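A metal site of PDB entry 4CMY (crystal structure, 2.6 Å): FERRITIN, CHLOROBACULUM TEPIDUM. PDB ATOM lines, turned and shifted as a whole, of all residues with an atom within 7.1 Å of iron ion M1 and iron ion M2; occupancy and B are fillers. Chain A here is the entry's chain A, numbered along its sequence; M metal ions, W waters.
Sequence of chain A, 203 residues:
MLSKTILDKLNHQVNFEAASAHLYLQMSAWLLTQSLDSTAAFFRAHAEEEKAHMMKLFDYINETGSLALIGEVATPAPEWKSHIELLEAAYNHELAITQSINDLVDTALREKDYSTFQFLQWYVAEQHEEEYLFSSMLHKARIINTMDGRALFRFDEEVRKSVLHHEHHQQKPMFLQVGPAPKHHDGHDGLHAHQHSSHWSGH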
ATOM      1  N   GLN A  13      27.493   2.909  32.833  1.00  0.00           N
ATOM      2  CA  GLN A  13      26.632   3.466  31.814  1.00  0.00           C
ATOM      3  C   GLN A  13      25.265   3.822  32.376  1.00  0.00           C
ATOM      4  O   GLN A  13      24.672   4.838  32.035  1.00  0.00           O
ATOM      5  CB  GLN A  13      26.501   2.470  30.680  1.00  0.00           C
ATOM      6  CG  GLN A  13      25.957   3.092  29.400  1.00  0.00           C
ATOM      7  CD  GLN A  13      26.895   4.088  28.800  1.00  0.00           C
ATOM      8  OE1 GLN A  13      28.112   3.934  28.892  1.00  0.00           O
ATOM      9  NE2 GLN A  13      26.353   5.122  28.186  1.00  0.00           N
ATOM     10  N   PHE A  16      25.800   7.045  33.874  1.00  0.00           N
ATOM     11  CA  PHE A  16      26.033   8.037  32.837  1.00  0.00           C
ATOM     12  C   PHE A  16      24.704   8.502  32.206  1.00  0.00           C
ATOM     13  O   PHE A  16      24.478   9.688  32.017  1.00  0.00           O
ATOM     14  CB  PHE A  16      26.956   7.428  31.763  1.00  0.00           C
ATOM     15  CG  PHE A  16      27.774   8.406  30.987  1.00  0.00           C
ATOM     16  CD1 PHE A  16      27.654   9.793  31.146  1.00  0.00           C
ATOM     17  CD2 PHE A  16      28.638   7.942  30.017  1.00  0.00           C
ATOM     18  CE1 PHE A  16      28.431  10.663  30.394  1.00  0.00           C
ATOM     19  CE2 PHE A  16      29.383   8.825  29.239  1.00  0.00           C
ATOM     20  CZ  PHE A  16      29.286  10.168  29.440  1.00  0.00           C
ATOM     21  N   GLU A  17      23.813   7.566  31.923  1.00  0.00           N
ATOM     22  CA  GLU A  17      22.499   7.918  31.379  1.00  0.00           C
ATOM     23  C   GLU A  17      21.688   8.706  32.397  1.00  0.00           C
ATOM     24  O   GLU A  17      21.060   9.712  32.060  1.00  0.00           O
ATOM     25  CB  GLU A  17      21.730   6.677  30.901  1.00  0.00           C
ATOM     26  CG  GLU A  17      22.457   5.854  29.854  1.00  0.00           C
ATOM     27  CD  GLU A  17      22.566   6.495  28.470  1.00  0.00           C
ATOM     28  OE1 GLU A  17      21.752   7.404  28.096  1.00  0.00           O
ATOM     29  OE2 GLU A  17      23.433   5.999  27.660  1.00  0.00           O
ATOM     30  N   SER A  20      22.877  12.169  32.357  1.00  0.00           N
ATOM     31  CA  SER A  20      22.431  12.864  31.155  1.00  0.00           C
ATOM     32  C   SER A  20      21.050  13.416  31.304  1.00  0.00           C
ATOM     33  O   SER A  20      20.783  14.523  30.937  1.00  0.00           O
ATOM     34  CB  SER A  20      22.457  11.926  29.943  1.00  0.00           C
ATOM     35  OG  SER A  20      23.729  11.332  29.827  1.00  0.00           O
ATOM     36  N   TYR A  24      20.290  17.380  31.122  1.00  0.00           N
ATOM     37  CA  TYR A  24      19.337  17.980  30.204  1.00  0.00           C
ATOM     38  C   TYR A  24      18.174  18.705  30.922  1.00  0.00           C
ATOM     39  O   TYR A  24      17.669  19.720  30.428  1.00  0.00           O
ATOM     40  CB  TYR A  24      18.845  16.955  29.209  1.00  0.00           C
ATOM     41  CG  TYR A  24      19.930  16.396  28.314  1.00  0.00           C
ATOM     42  CD1 TYR A  24      21.067  17.106  28.012  1.00  0.00           C
ATOM     43  CD2 TYR A  24      19.791  15.154  27.723  1.00  0.00           C
ATOM     44  CE1 TYR A  24      22.030  16.600  27.178  1.00  0.00           C
ATOM     45  CE2 TYR A  24      20.743  14.657  26.887  1.00  0.00           C
ATOM     46  CZ  TYR A  24      21.860  15.395  26.610  1.00  0.00           C
ATOM     47  OH  TYR A  24      22.843  14.875  25.758  1.00  0.00           O
ATOM     48  N   HIS A  46      13.868  15.444  26.179  1.00  0.00           N
ATOM     49  CA  HIS A  46      14.978  14.548  25.965  1.00  0.00           C
ATOM     50  C   HIS A  46      15.516  13.968  27.255  1.00  0.00           C
ATOM     51  O   HIS A  46      16.125  12.909  27.237  1.00  0.00           O
ATOM     52  CB  HIS A  46      16.095  15.209  25.172  1.00  0.00           C
ATOM     53  CG  HIS A  46      16.830  14.235  24.349  1.00  0.00           C
ATOM     54  ND1 HIS A  46      16.324  13.768  23.153  1.00  0.00           N
ATOM     55  CD2 HIS A  46      17.950  13.522  24.595  1.00  0.00           C
ATOM     56  CE1 HIS A  46      17.144  12.847  22.671  1.00  0.00           C
ATOM     57  NE2 HIS A  46      18.131  12.689  23.529  1.00  0.00           N
ATOM     58  N   GLU A  49      13.955  10.798  27.533  1.00  0.00           N
ATOM     59  CA  GLU A  49      14.563   9.784  26.692  1.00  0.00           C
ATOM     60  C   GLU A  49      15.775   9.167  27.384  1.00  0.00           C
ATOM     61  O   GLU A  49      15.972   7.959  27.314  1.00  0.00           O
ATOM     62  CB  GLU A  49      14.975  10.368  25.339  1.00  0.00           C
ATOM     63  CG  GLU A  49      13.820  10.531  24.369  1.00  0.00           C
ATOM     64  CD  GLU A  49      13.347   9.192  23.817  1.00  0.00           C
ATOM     65  OE1 GLU A  49      14.184   8.268  23.488  1.00  0.00           O
ATOM     66  OE2 GLU A  49      12.114   9.054  23.771  1.00  0.00           O
ATOM     67  N   GLU A  50      16.578   9.986  28.029  1.00  0.00           N
ATOM     68  CA  GLU A  50      17.761   9.493  28.709  1.00  0.00           C
ATOM     69  C   GLU A  50      17.378   8.601  29.872  1.00  0.00           C
ATOM     70  O   GLU A  50      18.047   7.627  30.162  1.00  0.00           O
ATOM     71  CB  GLU A  50      18.686  10.638  29.161  1.00  0.00           C
ATOM     72  CG  GLU A  50      19.212  11.470  27.997  1.00  0.00           C
ATOM     73  CD  GLU A  50      20.137  10.720  27.018  1.00  0.00           C
ATOM     74  OE1 GLU A  50      20.570   9.575  27.342  1.00  0.00           O
ATOM     75  OE2 GLU A  50      20.440  11.319  25.901  1.00  0.00           O
ATOM     76  N   LYS A  51      16.273   8.892  30.511  1.00  0.00           N
ATOM     77  CA  LYS A  51      15.778   8.013  31.532  1.00  0.00           C
ATOM     78  C   LYS A  51      15.380   6.678  31.039  1.00  0.00           C
ATOM     79  O   LYS A  51      15.647   5.691  31.690  1.00  0.00           O
ATOM     80  CB  LYS A  51      14.573   8.634  32.139  1.00  0.00           C
ATOM     81  CG  LYS A  51      14.577   8.335  33.556  1.00  0.00           C
ATOM     82  CD  LYS A  51      13.237   8.629  34.212  1.00  0.00           C
ATOM     83  CE  LYS A  51      12.632   7.297  34.500  1.00  0.00           C
ATOM     84  NZ  LYS A  51      11.633   7.283  35.585  1.00  0.00           N
ATOM     85  N   HIS A  53      16.791   5.263  28.475  1.00  0.00           N
ATOM     86  CA  HIS A  53      18.046   4.598  28.184  1.00  0.00           C
ATOM     87  C   HIS A  53      18.585   3.980  29.456  1.00  0.00           C
ATOM     88  O   HIS A  53      19.092   2.860  29.444  1.00  0.00           O
ATOM     89  CB  HIS A  53      19.103   5.538  27.637  1.00  0.00           C
ATOM     90  CG  HIS A  53      18.744   6.171  26.328  1.00  0.00           C
ATOM     91  ND1 HIS A  53      19.471   7.213  25.801  1.00  0.00           N
ATOM     92  CD2 HIS A  53      17.699   5.969  25.495  1.00  0.00           C
ATOM     93  CE1 HIS A  53      18.907   7.594  24.671  1.00  0.00           C
ATOM     94  NE2 HIS A  53      17.829   6.863  24.460  1.00  0.00           N
ATOM     95  N   MET A  54      18.485   4.725  30.544  1.00  0.00           N
ATOM     96  CA  MET A  54      18.951   4.251  31.841  1.00  0.00           C
ATOM     97  C   MET A  54      18.193   2.995  32.257  1.00  0.00           C
ATOM     98  O   MET A  54      18.829   2.008  32.636  1.00  0.00           O
ATOM     99  CB  MET A  54      18.786   5.337  32.892  1.00  0.00           C
ATOM    100  CG  MET A  54      19.184   4.887  34.279  1.00  0.00           C
ATOM    101  SD  MET A  54      18.690   6.082  35.543  1.00  0.00           S
ATOM    102  CE  MET A  54      16.979   5.652  35.668  1.00  0.00           C
ATOM    103  N   HIS A  93      28.812  16.008  25.146  1.00  0.00           N
ATOM    104  CA  HIS A  93      28.300  15.031  26.092  1.00  0.00           C
ATOM    105  C   HIS A  93      27.755  13.802  25.347  1.00  0.00           C
ATOM    106  O   HIS A  93      28.099  12.674  25.681  1.00  0.00           O
ATOM    107  CB  HIS A  93      27.212  15.670  26.939  1.00  0.00           C
ATOM    108  CG  HIS A  93      26.648  14.769  27.954  1.00  0.00           C
ATOM    109  ND1 HIS A  93      27.236  14.593  29.195  1.00  0.00           N
ATOM    110  CD2 HIS A  93      25.593  13.915  27.910  1.00  0.00           C
ATOM    111  CE1 HIS A  93      26.543  13.698  29.873  1.00  0.00           C
ATOM    112  NE2 HIS A  93      25.556  13.261  29.118  1.00  0.00           N
ATOM    113  N   GLU A  94      27.003  14.024  24.277  1.00  0.00           N
ATOM    114  CA  GLU A  94      26.564  12.905  23.458  1.00  0.00           C
ATOM    115  C   GLU A  94      27.720  12.134  22.785  1.00  0.00           C
ATOM    116  O   GLU A  94      27.658  10.911  22.686  1.00  0.00           O
ATOM    117  CB  GLU A  94      25.482  13.328  22.444  1.00  0.00           C
ATOM    118  CG  GLU A  94      24.131  13.631  23.097  1.00  0.00           C
ATOM    119  CD  GLU A  94      23.383  12.391  23.592  1.00  0.00           C
ATOM    120  OE1 GLU A  94      23.733  11.290  23.091  1.00  0.00           O
ATOM    121  OE2 GLU A  94      22.411  12.513  24.436  1.00  0.00           O
ATOM    122  N   ILE A  97      29.069   9.870  25.376  1.00  0.00           N
ATOM    123  CA  ILE A  97      28.205   8.726  25.595  1.00  0.00           C
ATOM    124  C   ILE A  97      28.501   7.703  24.533  1.00  0.00           C
ATOM    125  O   ILE A  97      28.640   6.531  24.818  1.00  0.00           O
ATOM    126  CB  ILE A  97      26.724   9.105  25.593  1.00  0.00           C
ATOM    127  CG1 ILE A  97      26.383   9.841  26.897  1.00  0.00           C
ATOM    128  CG2 ILE A  97      25.840   7.880  25.558  1.00  0.00           C
ATOM    129  CD1 ILE A  97      25.080  10.577  26.836  1.00  0.00           C
ATOM    130  N   ILE A 101      29.702   3.835  25.001  1.00  0.00           N
ATOM    131  CA  ILE A 101      28.994   2.702  24.438  1.00  0.00           C
ATOM    132  C   ILE A 101      29.935   1.900  23.549  1.00  0.00           C
ATOM    133  O   ILE A 101      29.951   0.663  23.625  1.00  0.00           O
ATOM    134  CB  ILE A 101      27.780   3.134  23.608  1.00  0.00           C
ATOM    135  CG1 ILE A 101      26.691   3.774  24.468  1.00  0.00           C
ATOM    136  CG2 ILE A 101      27.186   1.943  22.847  1.00  0.00           C
ATOM    137  CD1 ILE A 101      26.040   2.839  25.468  1.00  0.00           C
ATOM    138  N   TRP A 122      21.186  -1.928  20.125  1.00  0.00           N
ATOM    139  CA  TRP A 122      20.154  -0.900  20.268  1.00  0.00           C
ATOM    140  C   TRP A 122      20.790   0.470  20.573  1.00  0.00           C
ATOM    141  O   TRP A 122      20.428   1.467  19.946  1.00  0.00           O
ATOM    142  CB  TRP A 122      19.180  -1.275  21.366  1.00  0.00           C
ATOM    143  CG  TRP A 122      18.033  -0.396  21.405  1.00  0.00           C
ATOM    144  CD1 TRP A 122      16.906  -0.550  20.695  1.00  0.00           C
ATOM    145  CD2 TRP A 122      17.892   0.830  22.144  1.00  0.00           C
ATOM    146  NE1 TRP A 122      16.053   0.502  20.957  1.00  0.00           N
ATOM    147  CE2 TRP A 122      16.637   1.358  21.852  1.00  0.00           C
ATOM    148  CE3 TRP A 122      18.708   1.520  23.048  1.00  0.00           C
ATOM    149  CZ2 TRP A 122      16.149   2.525  22.405  1.00  0.00           C
ATOM    150  CZ3 TRP A 122      18.222   2.673  23.630  1.00  0.00           C
ATOM    151  CH2 TRP A 122      16.961   3.182  23.282  1.00  0.00           C
ATOM    152  N   TYR A 123      21.753   0.518  21.507  1.00  0.00           N
ATOM    153  CA  TYR A 123      22.422   1.773  21.901  1.00  0.00           C
ATOM    154  C   TYR A 123      23.324   2.328  20.819  1.00  0.00           C
ATOM    155  O   TYR A 123      23.421   3.530  20.659  1.00  0.00           O
ATOM    156  CB  TYR A 123      23.231   1.616  23.194  1.00  0.00           C
ATOM    157  CG  TYR A 123      22.354   1.480  24.387  1.00  0.00           C
ATOM    158  CD1 TYR A 123      21.812   0.263  24.718  1.00  0.00           C
ATOM    159  CD2 TYR A 123      21.992   2.585  25.136  1.00  0.00           C
ATOM    160  CE1 TYR A 123      20.951   0.130  25.777  1.00  0.00           C
ATOM    161  CE2 TYR A 123      21.130   2.453  26.209  1.00  0.00           C
ATOM    162  CZ  TYR A 123      20.612   1.205  26.524  1.00  0.00           C
ATOM    163  OH  TYR A 123      19.756   1.031  27.571  1.00  0.00           O
ATOM    164  N   GLU A 126      20.924   3.928  18.551  1.00  0.00           N
ATOM    165  CA  GLU A 126      20.343   5.104  19.163  1.00  0.00           C
ATOM    166  C   GLU A 126      21.328   6.251  19.201  1.00  0.00           C
ATOM    167  O   GLU A 126      20.953   7.400  18.983  1.00  0.00           O
ATOM    168  CB  GLU A 126      19.821   4.793  20.551  1.00  0.00           C
ATOM    169  CG  GLU A 126      18.912   5.892  21.159  1.00  0.00           C
ATOM    170  CD  GLU A 126      17.506   6.014  20.534  1.00  0.00           C
ATOM    171  OE1 GLU A 126      17.085   5.132  19.731  1.00  0.00           O
ATOM    172  OE2 GLU A 126      16.818   7.012  20.911  1.00  0.00           O
ATOM    173  N   GLN A 127      22.602   5.975  19.415  1.00  0.00           N
ATOM    174  CA  GLN A 127      23.595   7.064  19.521  1.00  0.00           C
ATOM    175  C   GLN A 127      23.896   7.695  18.180  1.00  0.00           C
ATOM    176  O   GLN A 127      24.219   8.848  18.114  1.00  0.00           O
ATOM    177  CB  GLN A 127      24.869   6.589  20.218  1.00  0.00           C
ATOM    178  CG  GLN A 127      24.621   6.443  21.697  1.00  0.00           C
ATOM    179  CD  GLN A 127      24.248   7.761  22.367  1.00  0.00           C
ATOM    180  OE1 GLN A 127      23.270   7.837  23.142  1.00  0.00           O
ATOM    181  NE2 GLN A 127      25.043   8.807  22.104  1.00  0.00           N
ATOM    182  N   GLU A 130      21.173  10.139  18.052  1.00  0.00           N
ATOM    183  CA  GLU A 130      21.439  11.237  19.002  1.00  0.00           C
ATOM    184  C   GLU A 130      22.479  12.203  18.466  1.00  0.00           C
ATOM    185  O   GLU A 130      22.321  13.406  18.548  1.00  0.00           O
ATOM    186  CB  GLU A 130      21.970  10.699  20.318  1.00  0.00           C
ATOM    187  CG  GLU A 130      21.020   9.847  21.121  1.00  0.00           C
ATOM    188  CD  GLU A 130      20.080  10.675  21.958  1.00  0.00           C
ATOM    189  OE1 GLU A 130      20.433  11.047  23.136  1.00  0.00           O
ATOM    190  OE2 GLU A 130      18.984  10.960  21.414  1.00  0.00           O
ATOM    191  N   GLU A 131      23.576  11.676  17.920  1.00  0.00           N
ATOM    192  CA  GLU A 131      24.593  12.548  17.351  1.00  0.00           C
ATOM    193  C   GLU A 131      24.063  13.346  16.162  1.00  0.00           C
ATOM    194  O   GLU A 131      24.397  14.518  16.009  1.00  0.00           O
ATOM    195  CB  GLU A 131      25.794  11.763  16.884  1.00  0.00           C
ATOM    196  CG  GLU A 131      26.679  11.349  18.046  1.00  0.00           C
ATOM    197  CD  GLU A 131      27.864  10.514  17.601  1.00  0.00           C
ATOM    198  OE1 GLU A 131      28.352  10.694  16.461  1.00  0.00           O
ATOM    199  OE2 GLU A 131      28.277   9.650  18.375  1.00  0.00           O
ATOM    200  N   PHE A 134      21.744  16.197  17.779  1.00  0.00           N
ATOM    201  CA  PHE A 134      22.468  17.265  18.491  1.00  0.00           C
ATOM    202  C   PHE A 134      23.497  18.007  17.626  1.00  0.00           C
ATOM    203  O   PHE A 134      23.636  19.209  17.756  1.00  0.00           O
ATOM    204  CB  PHE A 134      23.152  16.725  19.738  1.00  0.00           C
ATOM    205  CG  PHE A 134      22.203  16.470  20.866  1.00  0.00           C
ATOM    206  CD1 PHE A 134      21.556  15.262  20.999  1.00  0.00           C
ATOM    207  CD2 PHE A 134      21.903  17.462  21.751  1.00  0.00           C
ATOM    208  CE1 PHE A 134      20.658  15.046  22.002  1.00  0.00           C
ATOM    209  CE2 PHE A 134      20.993  17.254  22.752  1.00  0.00           C
ATOM    210  CZ  PHE A 134      20.380  16.033  22.897  1.00  0.00           C
HETATM  211 FE    FE M   1      21.634  10.623  24.571  1.00  0.00          FE
HETATM  212 FE    FE M   2      21.418   8.042  26.219  1.00  0.00          FE
HETATM  213  O   HOH W   1      22.354   6.207  25.455  1.00  0.00           O
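OH of Tyr 123 lies within hydrogen-bond range of O of His 53, 2.7 Å away. OE1 of Glu 94 sits at hydrogen-bond distance from NE2 of Gln 127, 3.0 Å away. OH of Tyr 24 sits close to OE2 of Glu 94 (2.7 Å). NE2 of Gln 13 sits at hydrogen-bond distance from OE2 of Glu 17, 3.1 Å away. The side-chain carboxylate (OE2) of Glu 130 lies within hydrogen-bond range of a ring nitrogen (NE2) of His 46.
Iron ion M1 is bound by the side-chain carboxylate (OE2) of Glu 50 (1.9 Å), the side-chain carboxylate (OE1) of Glu 130 (1.9 Å) and the side-chain carboxylate (OE2) of Glu 94 (2.0 Å). Iron ion M1 has three donor atoms within binding distance. Slightly farther from iron ion M1 lies the side-chain carboxylate (OE1) of Glu 94 (2.7 Å).
OE1 of Gln 127 touches iron ion M2 (3.6 Å).
Water W1 lies within hydrogen-bond range of the side-chain carboxylate (OE2) of Glu 17 (2.5 Å) and the side-chain amide oxygen (OE1) of Gln 127 (3.0 Å).
The side-chain carboxylate (OE1) of Glu 17 binds iron ion M2 (2.0 Å). Iron ion M2 is bound by OE1 of Glu 50 (2.1 Å). A ring nitrogen (ND1) of His 53 is bound to iron ion M2, at 2.2 Å. Water W1 is bound to iron ion M2 (2.2 Å).
OE1 of Gln 127 touches iron ion M1, 3.5 Å away. Of the 22 residues printed, 4 come within 4 Å of iron ion M1.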
